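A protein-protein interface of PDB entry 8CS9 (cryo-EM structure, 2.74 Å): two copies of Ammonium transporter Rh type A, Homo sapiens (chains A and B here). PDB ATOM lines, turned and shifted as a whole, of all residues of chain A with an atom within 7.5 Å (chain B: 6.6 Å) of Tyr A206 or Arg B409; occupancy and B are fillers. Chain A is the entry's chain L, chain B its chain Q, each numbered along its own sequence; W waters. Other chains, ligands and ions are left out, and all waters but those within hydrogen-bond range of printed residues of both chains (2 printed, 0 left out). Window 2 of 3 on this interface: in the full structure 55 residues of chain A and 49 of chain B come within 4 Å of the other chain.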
ATOM      1  N   THR A  70       2.888 -18.948  -9.790  1.00  0.00           N
ATOM      2  CA  THR A  70       2.266 -17.978  -8.900  1.00  0.00           C
ATOM      3  C   THR A  70       2.864 -17.986  -7.500  1.00  0.00           C
ATOM      4  O   THR A  70       2.217 -17.511  -6.561  1.00  0.00           O
ATOM      5  CB  THR A  70       0.755 -18.220  -8.817  1.00  0.00           C
ATOM      6  OG1 THR A  70       0.501 -19.565  -8.395  1.00  0.00           O
ATOM      7  CG2 THR A  70       0.103 -17.983 -10.168  1.00  0.00           C
ATOM      8  N   PHE A  71       4.077 -18.518  -7.336  1.00  0.00           N
ATOM      9  CA  PHE A  71       4.708 -18.538  -6.022  1.00  0.00           C
ATOM     10  C   PHE A  71       5.167 -17.151  -5.595  1.00  0.00           C
ATOM     11  O   PHE A  71       5.228 -16.868  -4.395  1.00  0.00           O
ATOM     12  CB  PHE A  71       5.883 -19.519  -6.018  1.00  0.00           C
ATOM     13  CG  PHE A  71       7.070 -19.056  -6.816  1.00  0.00           C
ATOM     14  CD1 PHE A  71       7.092 -19.195  -8.192  1.00  0.00           C
ATOM     15  CD2 PHE A  71       8.168 -18.495  -6.188  1.00  0.00           C
ATOM     16  CE1 PHE A  71       8.180 -18.774  -8.926  1.00  0.00           C
ATOM     17  CE2 PHE A  71       9.258 -18.073  -6.920  1.00  0.00           C
ATOM     18  CZ  PHE A  71       9.262 -18.214  -8.291  1.00  0.00           C
ATOM     19  N   SER A 203       8.511 -15.477  -1.995  1.00  0.00           N
ATOM     20  CA  SER A 203       7.222 -16.145  -1.998  1.00  0.00           C
ATOM     21  C   SER A 203       6.415 -15.773  -0.757  1.00  0.00           C
ATOM     22  O   SER A 203       6.945 -15.309   0.252  1.00  0.00           O
ATOM     23  CB  SER A 203       7.403 -17.659  -2.082  1.00  0.00           C
ATOM     24  OG  SER A 203       7.995 -18.170  -0.904  1.00  0.00           O
ATOM     25  N   ALA A 204       5.108 -15.983  -0.847  1.00  0.00           N
ATOM     26  CA  ALA A 204       4.203 -15.853   0.282  1.00  0.00           C
ATOM     27  C   ALA A 204       3.613 -17.217   0.609  1.00  0.00           C
ATOM     28  O   ALA A 204       3.853 -18.209  -0.084  1.00  0.00           O
ATOM     29  CB  ALA A 204       3.092 -14.834  -0.005  1.00  0.00           C
ATOM     30  N   TYR A 205       2.832 -17.261   1.688  1.00  0.00           N
ATOM     31  CA  TYR A 205       2.280 -18.525   2.164  1.00  0.00           C
ATOM     32  C   TYR A 205       1.165 -19.018   1.243  1.00  0.00           C
ATOM     33  O   TYR A 205       1.228 -20.129   0.693  1.00  0.00           O
ATOM     34  CB  TYR A 205       1.781 -18.346   3.599  1.00  0.00           C
ATOM     35  CG  TYR A 205       1.327 -19.616   4.266  1.00  0.00           C
ATOM     36  CD1 TYR A 205       2.230 -20.627   4.559  1.00  0.00           C
ATOM     37  CD2 TYR A 205      -0.003 -19.805   4.610  1.00  0.00           C
ATOM     38  CE1 TYR A 205       1.822 -21.792   5.161  1.00  0.00           C
ATOM     39  CE2 TYR A 205      -0.420 -20.966   5.218  1.00  0.00           C
ATOM     40  CZ  TYR A 205       0.497 -21.955   5.491  1.00  0.00           C
ATOM     41  OH  TYR A 205       0.087 -23.115   6.095  1.00  0.00           O
ATOM     42  N   TYR A 206       0.136 -18.192   1.051  1.00  0.00           N
ATOM     43  CA  TYR A 206      -0.949 -18.558   0.150  1.00  0.00           C
ATOM     44  C   TYR A 206      -0.478 -18.623  -1.296  1.00  0.00           C
ATOM     45  O   TYR A 206      -1.068 -19.345  -2.105  1.00  0.00           O
ATOM     46  CB  TYR A 206      -2.103 -17.571   0.298  1.00  0.00           C
ATOM     47  CG  TYR A 206      -2.740 -17.581   1.667  1.00  0.00           C
ATOM     48  CD1 TYR A 206      -2.786 -18.743   2.425  1.00  0.00           C
ATOM     49  CD2 TYR A 206      -3.287 -16.424   2.207  1.00  0.00           C
ATOM     50  CE1 TYR A 206      -3.364 -18.755   3.676  1.00  0.00           C
ATOM     51  CE2 TYR A 206      -3.869 -16.428   3.459  1.00  0.00           C
ATOM     52  CZ  TYR A 206      -3.903 -17.596   4.189  1.00  0.00           C
ATOM     53  OH  TYR A 206      -4.481 -17.604   5.435  1.00  0.00           O
ATOM     54  N   SER A 207       0.589 -17.896  -1.634  1.00  0.00           N
ATOM     55  CA  SER A 207       1.160 -17.994  -2.974  1.00  0.00           C
ATOM     56  C   SER A 207       1.718 -19.388  -3.236  1.00  0.00           C
ATOM     57  O   SER A 207       1.504 -19.960  -4.310  1.00  0.00           O
ATOM     58  CB  SER A 207       2.246 -16.935  -3.154  1.00  0.00           C
ATOM     59  OG  SER A 207       1.687 -15.678  -3.477  1.00  0.00           O
ATOM     60  N   ASP A 208       2.431 -19.959  -2.260  1.00  0.00           N
ATOM     61  CA  ASP A 208       2.915 -21.327  -2.414  1.00  0.00           C
ATOM     62  C   ASP A 208       1.768 -22.329  -2.374  1.00  0.00           C
ATOM     63  O   ASP A 208       1.814 -23.354  -3.071  1.00  0.00           O
ATOM     64  CB  ASP A 208       3.951 -21.643  -1.337  1.00  0.00           C
ATOM     65  CG  ASP A 208       5.224 -20.838  -1.501  1.00  0.00           C
ATOM     66  OD1 ASP A 208       5.591 -20.531  -2.653  1.00  0.00           O
ATOM     67  OD2 ASP A 208       5.859 -20.506  -0.479  1.00  0.00           O
ATOM     68  N   LEU A 209       0.727 -22.042  -1.586  1.00  0.00           N
ATOM     69  CA  LEU A 209      -0.470 -22.878  -1.628  1.00  0.00           C
ATOM     70  C   LEU A 209      -1.077 -22.904  -3.029  1.00  0.00           C
ATOM     71  O   LEU A 209      -1.515 -23.956  -3.506  1.00  0.00           O
ATOM     72  CB  LEU A 209      -1.492 -22.381  -0.608  1.00  0.00           C
ATOM     73  CG  LEU A 209      -2.824 -23.128  -0.526  1.00  0.00           C
ATOM     74  CD1 LEU A 209      -2.604 -24.602  -0.231  1.00  0.00           C
ATOM     75  CD2 LEU A 209      -3.722 -22.495   0.523  1.00  0.00           C
ATOM     76  N   PHE A 210      -1.112 -21.751  -3.699  1.00  0.00           N
ATOM     77  CA  PHE A 210      -1.610 -21.698  -5.070  1.00  0.00           C
ATOM     78  C   PHE A 210      -0.668 -22.388  -6.048  1.00  0.00           C
ATOM     79  O   PHE A 210      -1.128 -23.001  -7.017  1.00  0.00           O
ATOM     80  CB  PHE A 210      -1.839 -20.247  -5.490  1.00  0.00           C
ATOM     81  CG  PHE A 210      -3.246 -19.777  -5.287  1.00  0.00           C
ATOM     82  CD1 PHE A 210      -4.197 -19.955  -6.274  1.00  0.00           C
ATOM     83  CD2 PHE A 210      -3.621 -19.160  -4.105  1.00  0.00           C
ATOM     84  CE1 PHE A 210      -5.493 -19.530  -6.089  1.00  0.00           C
ATOM     85  CE2 PHE A 210      -4.918 -18.730  -3.916  1.00  0.00           C
ATOM     86  CZ  PHE A 210      -5.852 -18.915  -4.910  1.00  0.00           C
ATOM     87  N   ALA A 211       0.644 -22.288  -5.827  1.00  0.00           N
ATOM     88  CA  ALA A 211       1.596 -22.954  -6.713  1.00  0.00           C
ATOM     89  C   ALA A 211       1.486 -24.471  -6.621  1.00  0.00           C
ATOM     90  O   ALA A 211       1.783 -25.182  -7.595  1.00  0.00           O
ATOM     91  CB  ALA A 211       3.016 -22.498  -6.393  1.00  0.00           C
ATOM     92  N   MET A 212       1.069 -24.978  -5.459  1.00  0.00           N
ATOM     93  CA  MET A 212       0.853 -26.413  -5.319  1.00  0.00           C
ATOM     94  C   MET A 212      -0.237 -26.919  -6.259  1.00  0.00           C
ATOM     95  O   MET A 212      -0.204 -28.085  -6.661  1.00  0.00           O
ATOM     96  CB  MET A 212       0.511 -26.755  -3.870  1.00  0.00           C
ATOM     97  CG  MET A 212       1.726 -27.023  -2.999  1.00  0.00           C
ATOM     98  SD  MET A 212       3.094 -27.775  -3.902  1.00  0.00           S
ATOM     99  CE  MET A 212       2.576 -29.487  -3.954  1.00  0.00           C
ATOM    100  N   ILE A 213      -1.196 -26.064  -6.631  1.00  0.00           N
ATOM    101  CA  ILE A 213      -2.226 -26.459  -7.593  1.00  0.00           C
ATOM    102  C   ILE A 213      -1.594 -26.817  -8.932  1.00  0.00           C
ATOM    103  O   ILE A 213      -1.866 -27.879  -9.510  1.00  0.00           O
ATOM    104  CB  ILE A 213      -3.268 -25.336  -7.759  1.00  0.00           C
ATOM    105  CG1 ILE A 213      -4.127 -25.194  -6.506  1.00  0.00           C
ATOM    106  CG2 ILE A 213      -4.141 -25.587  -8.977  1.00  0.00           C
ATOM    107  CD1 ILE A 213      -4.825 -23.860  -6.392  1.00  0.00           C
ATOM    108  N   THR A 408      -6.292  -5.095  -1.090  1.00  0.00           N
ATOM    109  CA  THR A 408      -6.040  -6.098  -0.066  1.00  0.00           C
ATOM    110  C   THR A 408      -5.760  -7.446  -0.717  1.00  0.00           C
ATOM    111  O   THR A 408      -6.162  -7.708  -1.852  1.00  0.00           O
ATOM    112  CB  THR A 408      -7.224  -6.231   0.908  1.00  0.00           C
ATOM    113  OG1 THR A 408      -8.373  -6.723   0.208  1.00  0.00           O
ATOM    114  CG2 THR A 408      -7.557  -4.887   1.539  1.00  0.00           C
ATOM    115  N   ARG A 409      -5.065  -8.300   0.025  1.00  0.00           N
ATOM    116  CA  ARG A 409      -4.709  -9.631  -0.452  1.00  0.00           C
ATOM    117  C   ARG A 409      -5.864 -10.613  -0.284  1.00  0.00           C
ATOM    118  O   ARG A 409      -5.979 -11.591  -1.021  1.00  0.00           O
ATOM    119  CB  ARG A 409      -3.473 -10.150   0.285  1.00  0.00           C
ATOM    120  CG  ARG A 409      -2.338  -9.149   0.385  1.00  0.00           C
ATOM    121  CD  ARG A 409      -1.411  -9.245  -0.809  1.00  0.00           C
ATOM    122  NE  ARG A 409      -0.719 -10.527  -0.858  1.00  0.00           N
ATOM    123  CZ  ARG A 409       0.129 -10.882  -1.812  1.00  0.00           C
ATOM    124  NH1 ARG A 409       0.425 -10.069  -2.811  1.00  0.00           N
ATOM    125  NH2 ARG A 409       0.695 -12.083  -1.761  1.00  0.00           N
ATOM    126  OXT ARG A 409      -6.710 -10.456   0.596  1.00  0.00           O
ATOM    127  N   LEU B  72     -15.112 -11.717  -5.607  1.00  0.00           N
ATOM    128  CA  LEU B  72     -15.512 -10.835  -4.519  1.00  0.00           C
ATOM    129  C   LEU B  72     -14.779 -11.205  -3.234  1.00  0.00           C
ATOM    130  O   LEU B  72     -14.645 -12.382  -2.892  1.00  0.00           O
ATOM    131  CB  LEU B  72     -17.024 -10.908  -4.314  1.00  0.00           C
ATOM    132  CG  LEU B  72     -17.875 -10.227  -5.387  1.00  0.00           C
ATOM    133  CD1 LEU B  72     -19.334 -10.595  -5.221  1.00  0.00           C
ATOM    134  CD2 LEU B  72     -17.692  -8.720  -5.347  1.00  0.00           C
ATOM    135  N   LYS B  73     -14.304 -10.184  -2.516  1.00  0.00           N
ATOM    136  CA  LYS B  73     -13.405 -10.428  -1.392  1.00  0.00           C
ATOM    137  C   LYS B  73     -14.126 -11.030  -0.189  1.00  0.00           C
ATOM    138  O   LYS B  73     -13.515 -11.785   0.575  1.00  0.00           O
ATOM    139  CB  LYS B  73     -12.683  -9.136  -1.001  1.00  0.00           C
ATOM    140  CG  LYS B  73     -13.569  -8.059  -0.406  1.00  0.00           C
ATOM    141  CD  LYS B  73     -12.747  -6.932   0.192  1.00  0.00           C
ATOM    142  CE  LYS B  73     -13.573  -5.664   0.342  1.00  0.00           C
ATOM    143  NZ  LYS B  73     -14.578  -5.769   1.428  1.00  0.00           N
ATOM    144  N   LYS B  74     -15.409 -10.720   0.001  1.00  0.00           N
ATOM    145  CA  LYS B  74     -16.171 -11.266   1.119  1.00  0.00           C
ATOM    146  C   LYS B  74     -17.318 -12.157   0.664  1.00  0.00           C
ATOM    147  O   LYS B  74     -18.280 -12.344   1.413  1.00  0.00           O
ATOM    148  CB  LYS B  74     -16.714 -10.147   2.011  1.00  0.00           C
ATOM    149  CG  LYS B  74     -15.774  -8.987   2.231  1.00  0.00           C
ATOM    150  CD  LYS B  74     -16.371  -7.984   3.199  1.00  0.00           C
ATOM    151  CE  LYS B  74     -15.687  -8.046   4.553  1.00  0.00           C
ATOM    152  NZ  LYS B  74     -16.516  -7.420   5.618  1.00  0.00           N
ATOM    153  N   SER B 203     -12.681  -6.681  -5.542  1.00  0.00           N
ATOM    154  CA  SER B 203     -11.928  -7.923  -5.564  1.00  0.00           C
ATOM    155  C   SER B 203     -10.742  -7.864  -4.607  1.00  0.00           C
ATOM    156  O   SER B 203     -10.419  -6.825  -4.030  1.00  0.00           O
ATOM    157  CB  SER B 203     -11.450  -8.233  -6.982  1.00  0.00           C
ATOM    158  OG  SER B 203     -10.389  -7.379  -7.362  1.00  0.00           O
ATOM    159  N   ALA B 204     -10.099  -9.015  -4.437  1.00  0.00           N
ATOM    160  CA  ALA B 204      -8.859  -9.138  -3.690  1.00  0.00           C
ATOM    161  C   ALA B 204      -7.869  -9.943  -4.520  1.00  0.00           C
ATOM    162  O   ALA B 204      -8.203 -10.486  -5.574  1.00  0.00           O
ATOM    163  CB  ALA B 204      -9.083  -9.790  -2.321  1.00  0.00           C
ATOM    164  N   TYR B 205      -6.631 -10.008  -4.030  1.00  0.00           N
ATOM    165  CA  TYR B 205      -5.556 -10.656  -4.775  1.00  0.00           C
ATOM    166  C   TYR B 205      -5.811 -12.154  -4.929  1.00  0.00           C
ATOM    167  O   TYR B 205      -5.938 -12.670  -6.048  1.00  0.00           O
ATOM    168  CB  TYR B 205      -4.228 -10.386  -4.064  1.00  0.00           C
ATOM    169  CG  TYR B 205      -3.002 -10.962  -4.728  1.00  0.00           C
ATOM    170  CD1 TYR B 205      -2.413 -10.328  -5.813  1.00  0.00           C
ATOM    171  CD2 TYR B 205      -2.418 -12.128  -4.254  1.00  0.00           C
ATOM    172  CE1 TYR B 205      -1.286 -10.848  -6.415  1.00  0.00           C
ATOM    173  CE2 TYR B 205      -1.294 -12.653  -4.850  1.00  0.00           C
ATOM    174  CZ  TYR B 205      -0.733 -12.011  -5.929  1.00  0.00           C
ATOM    175  OH  TYR B 205       0.387 -12.537  -6.522  1.00  0.00           O
ATOM    176  N   TYR B 206      -5.912 -12.866  -3.807  1.00  0.00           N
ATOM    177  CA  TYR B 206      -6.123 -14.307  -3.853  1.00  0.00           C
ATOM    178  C   TYR B 206      -7.525 -14.662  -4.331  1.00  0.00           C
ATOM    179  O   TYR B 206      -7.720 -15.721  -4.939  1.00  0.00           O
ATOM    180  CB  TYR B 206      -5.835 -14.907  -2.478  1.00  0.00           C
ATOM    181  CG  TYR B 206      -4.375 -14.812  -2.103  1.00  0.00           C
ATOM    182  CD1 TYR B 206      -3.397 -15.374  -2.913  1.00  0.00           C
ATOM    183  CD2 TYR B 206      -3.970 -14.134  -0.960  1.00  0.00           C
ATOM    184  CE1 TYR B 206      -2.061 -15.282  -2.584  1.00  0.00           C
ATOM    185  CE2 TYR B 206      -2.635 -14.037  -0.624  1.00  0.00           C
ATOM    186  CZ  TYR B 206      -1.686 -14.613  -1.440  1.00  0.00           C
ATOM    187  OH  TYR B 206      -0.354 -14.521  -1.114  1.00  0.00           O
ATOM    188  N   SER B 207      -8.502 -13.784  -4.090  1.00  0.00           N
ATOM    189  CA  SER B 207      -9.824 -13.976  -4.676  1.00  0.00           C
ATOM    190  C   SER B 207      -9.754 -13.937  -6.196  1.00  0.00           C
ATOM    191  O   SER B 207     -10.382 -14.756  -6.878  1.00  0.00           O
ATOM    192  CB  SER B 207     -10.788 -12.911  -4.154  1.00  0.00           C
ATOM    193  OG  SER B 207     -11.080 -13.106  -2.784  1.00  0.00           O
ATOM    194  N   ASP B 208      -8.971 -13.006  -6.746  1.00  0.00           N
ATOM    195  CA  ASP B 208      -8.788 -12.957  -8.190  1.00  0.00           C
ATOM    196  C   ASP B 208      -7.999 -14.155  -8.702  1.00  0.00           C
ATOM    197  O   ASP B 208      -8.211 -14.589  -9.837  1.00  0.00           O
ATOM    198  CB  ASP B 208      -8.099 -11.656  -8.593  1.00  0.00           C
ATOM    199  CG  ASP B 208      -9.055 -10.485  -8.650  1.00  0.00           C
ATOM    200  OD1 ASP B 208     -10.254 -10.709  -8.906  1.00  0.00           O
ATOM    201  OD2 ASP B 208      -8.603  -9.338  -8.452  1.00  0.00           O
ATOM    202  N   LEU B 209      -7.100 -14.713  -7.888  1.00  0.00           N
ATOM    203  CA  LEU B 209      -6.410 -15.933  -8.311  1.00  0.00           C
ATOM    204  C   LEU B 209      -7.366 -17.126  -8.377  1.00  0.00           C
ATOM    205  O   LEU B 209      -7.297 -17.943  -9.307  1.00  0.00           O
ATOM    206  CB  LEU B 209      -5.233 -16.216  -7.380  1.00  0.00           C
ATOM    207  CG  LEU B 209      -4.008 -15.322  -7.603  1.00  0.00           C
ATOM    208  CD1 LEU B 209      -2.841 -15.752  -6.730  1.00  0.00           C
ATOM    209  CD2 LEU B 209      -3.602 -15.292  -9.069  1.00  0.00           C
ATOM    210  N   PHE B 210      -8.279 -17.236  -7.408  1.00  0.00           N
ATOM    211  CA  PHE B 210      -9.322 -18.261  -7.489  1.00  0.00           C
ATOM    212  C   PHE B 210     -10.220 -18.036  -8.706  1.00  0.00           C
ATOM    213  O   PHE B 210     -10.631 -18.992  -9.388  1.00  0.00           O
ATOM    214  CB  PHE B 210     -10.153 -18.263  -6.205  1.00  0.00           C
ATOM    215  CG  PHE B 210      -9.495 -18.965  -5.049  1.00  0.00           C
ATOM    216  CD1 PHE B 210      -9.203 -20.316  -5.112  1.00  0.00           C
ATOM    217  CD2 PHE B 210      -9.187 -18.272  -3.889  1.00  0.00           C
ATOM    218  CE1 PHE B 210      -8.604 -20.960  -4.044  1.00  0.00           C
ATOM    219  CE2 PHE B 210      -8.589 -18.910  -2.822  1.00  0.00           C
ATOM    220  CZ  PHE B 210      -8.297 -20.257  -2.899  1.00  0.00           C
ATOM    221  N   PRO B 406     -14.420 -17.557   8.762  1.00  0.00           N
ATOM    222  CA  PRO B 406     -13.271 -17.568   9.672  1.00  0.00           C
ATOM    223  C   PRO B 406     -12.766 -16.160   9.944  1.00  0.00           C
ATOM    224  O   PRO B 406     -12.840 -15.272   9.093  1.00  0.00           O
ATOM    225  CB  PRO B 406     -12.227 -18.400   8.918  1.00  0.00           C
ATOM    226  CG  PRO B 406     -13.003 -19.186   7.918  1.00  0.00           C
ATOM    227  CD  PRO B 406     -14.166 -18.335   7.539  1.00  0.00           C
ATOM    228  N   LYS B 407     -12.260 -15.961  11.163  1.00  0.00           N
ATOM    229  CA  LYS B 407     -11.716 -14.660  11.538  1.00  0.00           C
ATOM    230  C   LYS B 407     -10.490 -14.316  10.700  1.00  0.00           C
ATOM    231  O   LYS B 407     -10.314 -13.166  10.282  1.00  0.00           O
ATOM    232  CB  LYS B 407     -11.384 -14.649  13.030  1.00  0.00           C
ATOM    233  CG  LYS B 407     -10.291 -13.673  13.437  1.00  0.00           C
ATOM    234  CD  LYS B 407      -9.257 -14.341  14.325  1.00  0.00           C
ATOM    235  CE  LYS B 407      -8.051 -13.442  14.542  1.00  0.00           C
ATOM    236  NZ  LYS B 407      -7.285 -13.826  15.759  1.00  0.00           N
ATOM    237  N   THR B 408      -9.644 -15.306  10.428  1.00  0.00           N
ATOM    238  CA  THR B 408      -8.443 -15.116   9.631  1.00  0.00           C
ATOM    239  C   THR B 408      -8.758 -15.261   8.148  1.00  0.00           C
ATOM    240  O   THR B 408      -9.456 -16.192   7.736  1.00  0.00           O
ATOM    241  CB  THR B 408      -7.371 -16.130  10.037  1.00  0.00           C
ATOM    242  OG1 THR B 408      -7.102 -16.007  11.438  1.00  0.00           O
ATOM    243  CG2 THR B 408      -6.085 -15.903   9.260  1.00  0.00           C
ATOM    244  N   ARG B 409      -8.239 -14.335   7.350  1.00  0.00           N
ATOM    245  CA  ARG B 409      -8.383 -14.409   5.902  1.00  0.00           C
ATOM    246  C   ARG B 409      -7.422 -15.441   5.313  1.00  0.00           C
ATOM    247  O   ARG B 409      -7.804 -16.267   4.487  1.00  0.00           O
ATOM    248  CB  ARG B 409      -8.140 -13.039   5.269  1.00  0.00           C
ATOM    249  CG  ARG B 409      -7.827 -13.085   3.782  1.00  0.00           C
ATOM    250  CD  ARG B 409      -8.761 -12.197   2.989  1.00  0.00           C
ATOM    251  NE  ARG B 409      -8.486 -12.264   1.560  1.00  0.00           N
ATOM    252  CZ  ARG B 409      -9.346 -12.701   0.651  1.00  0.00           C
ATOM    253  NH1 ARG B 409     -10.555 -13.116   0.989  1.00  0.00           N
ATOM    254  NH2 ARG B 409      -8.983 -12.723  -0.628  1.00  0.00           N
ATOM    255  OXT ARG B 409      -6.241 -15.481   5.657  1.00  0.00           O
HETATM  256  O   HOH W   1       1.208 -15.261  -5.834  1.00  0.00           O
HETATM  257  O   HOH W   2       0.097 -15.433   2.098  1.00  0.00           O
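The chain-end carboxylate (OXT) of Arg B409 sits at hydrogen-bond distance from the side-chain hydroxyl (OH) of Tyr A206 (2.8 Å). OG of Ser A207 lies within hydrogen-bond range of OH of Tyr B206, 3.3 Å away. O of Thr A408 lies within hydrogen-bond range of N of Tyr B205 (3.2 Å). O of Arg A409 sits at hydrogen-bond distance from N of Tyr B205. NH2 of Arg A409 sits at hydrogen-bond distance from OH of Tyr B206, 2.7 Å away. OXT of Arg A409 is in salt-bridge range of NE of Arg B409.
Among the printed residues, merely in contact across the chains: Ala A204 with Tyr B206, Tyr A206 with Tyr B206, Phe A210 with Tyr B206, Phe A210 with Leu B209, Phe A210 with Phe B210, Thr A408 with Ala B204 and Arg A409 with Ala B204.
The backbone carbonyl oxygen (O) of Lys B73 lies within hydrogen-bond range of the guanidinium group (NH1) of Arg B409 (3.3 Å). The side-chain hydroxyl (OG) of Ser B207 is in hydrogen-bond range of the guanidinium group (NH2) of Arg B409, 3.0 Å away.
Water W1 lies within hydrogen-bond range of OG of Ser A207 (2.4 Å), O of Thr A70 (2.6 Å) and OH of Tyr B205 (2.9 Å). Water W2 lies within hydrogen-bond range of the backbone NH (N) of Tyr A206, the backbone NH (N) of Tyr A205 and the side-chain hydroxyl (OH) of Tyr B206.
Of the printed residues of chain B, Tyr A206 touches Tyr B206 and Arg B409. Printed residues of chain B within 4 Å of Phe A210: Tyr B206, Leu B209 and Phe B210. Ile A213 touches none of the printed residues of chain B. Printed residues of chain A within 4 Å of Ala B204: Thr A408 (3.6 Å) and Arg A409 (3.8 Å). Arg B409 touches two residues of chain A. The nearest printed residue of chain A that does not touch Leu B209 is Thr A70 (4.7 Å).
Hydrophobic or aromatic side chains of chain B that line the printed part of chain A: Ala B204, Tyr B205, Tyr B206, Leu B209 and Phe B210. Hydrophobic or aromatic side chains of chain A within 4 Å of the printed part of chain B: Ala A204, Tyr A206 and Phe A210. Among the printed residues, no Asp or Glu carboxylate lies within 4 Å of a Lys or Arg side-chain nitrogen of the other chain.
Tyr A206 touches Arg B409, and with the chains exchanged Arg A409 touches Tyr B206. Ser A207 touches Tyr B206, but with the chains exchanged Tyr A206 does not touch Ser B207 (8.6 Å). Phe B210 touches its own counterpart, Phe A210. Arg B409 touches its own counterpart, Arg A409. Positions printed for both chains: 203, 204, 205, 206, 207, 208, 209, 210, 408 and 409.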
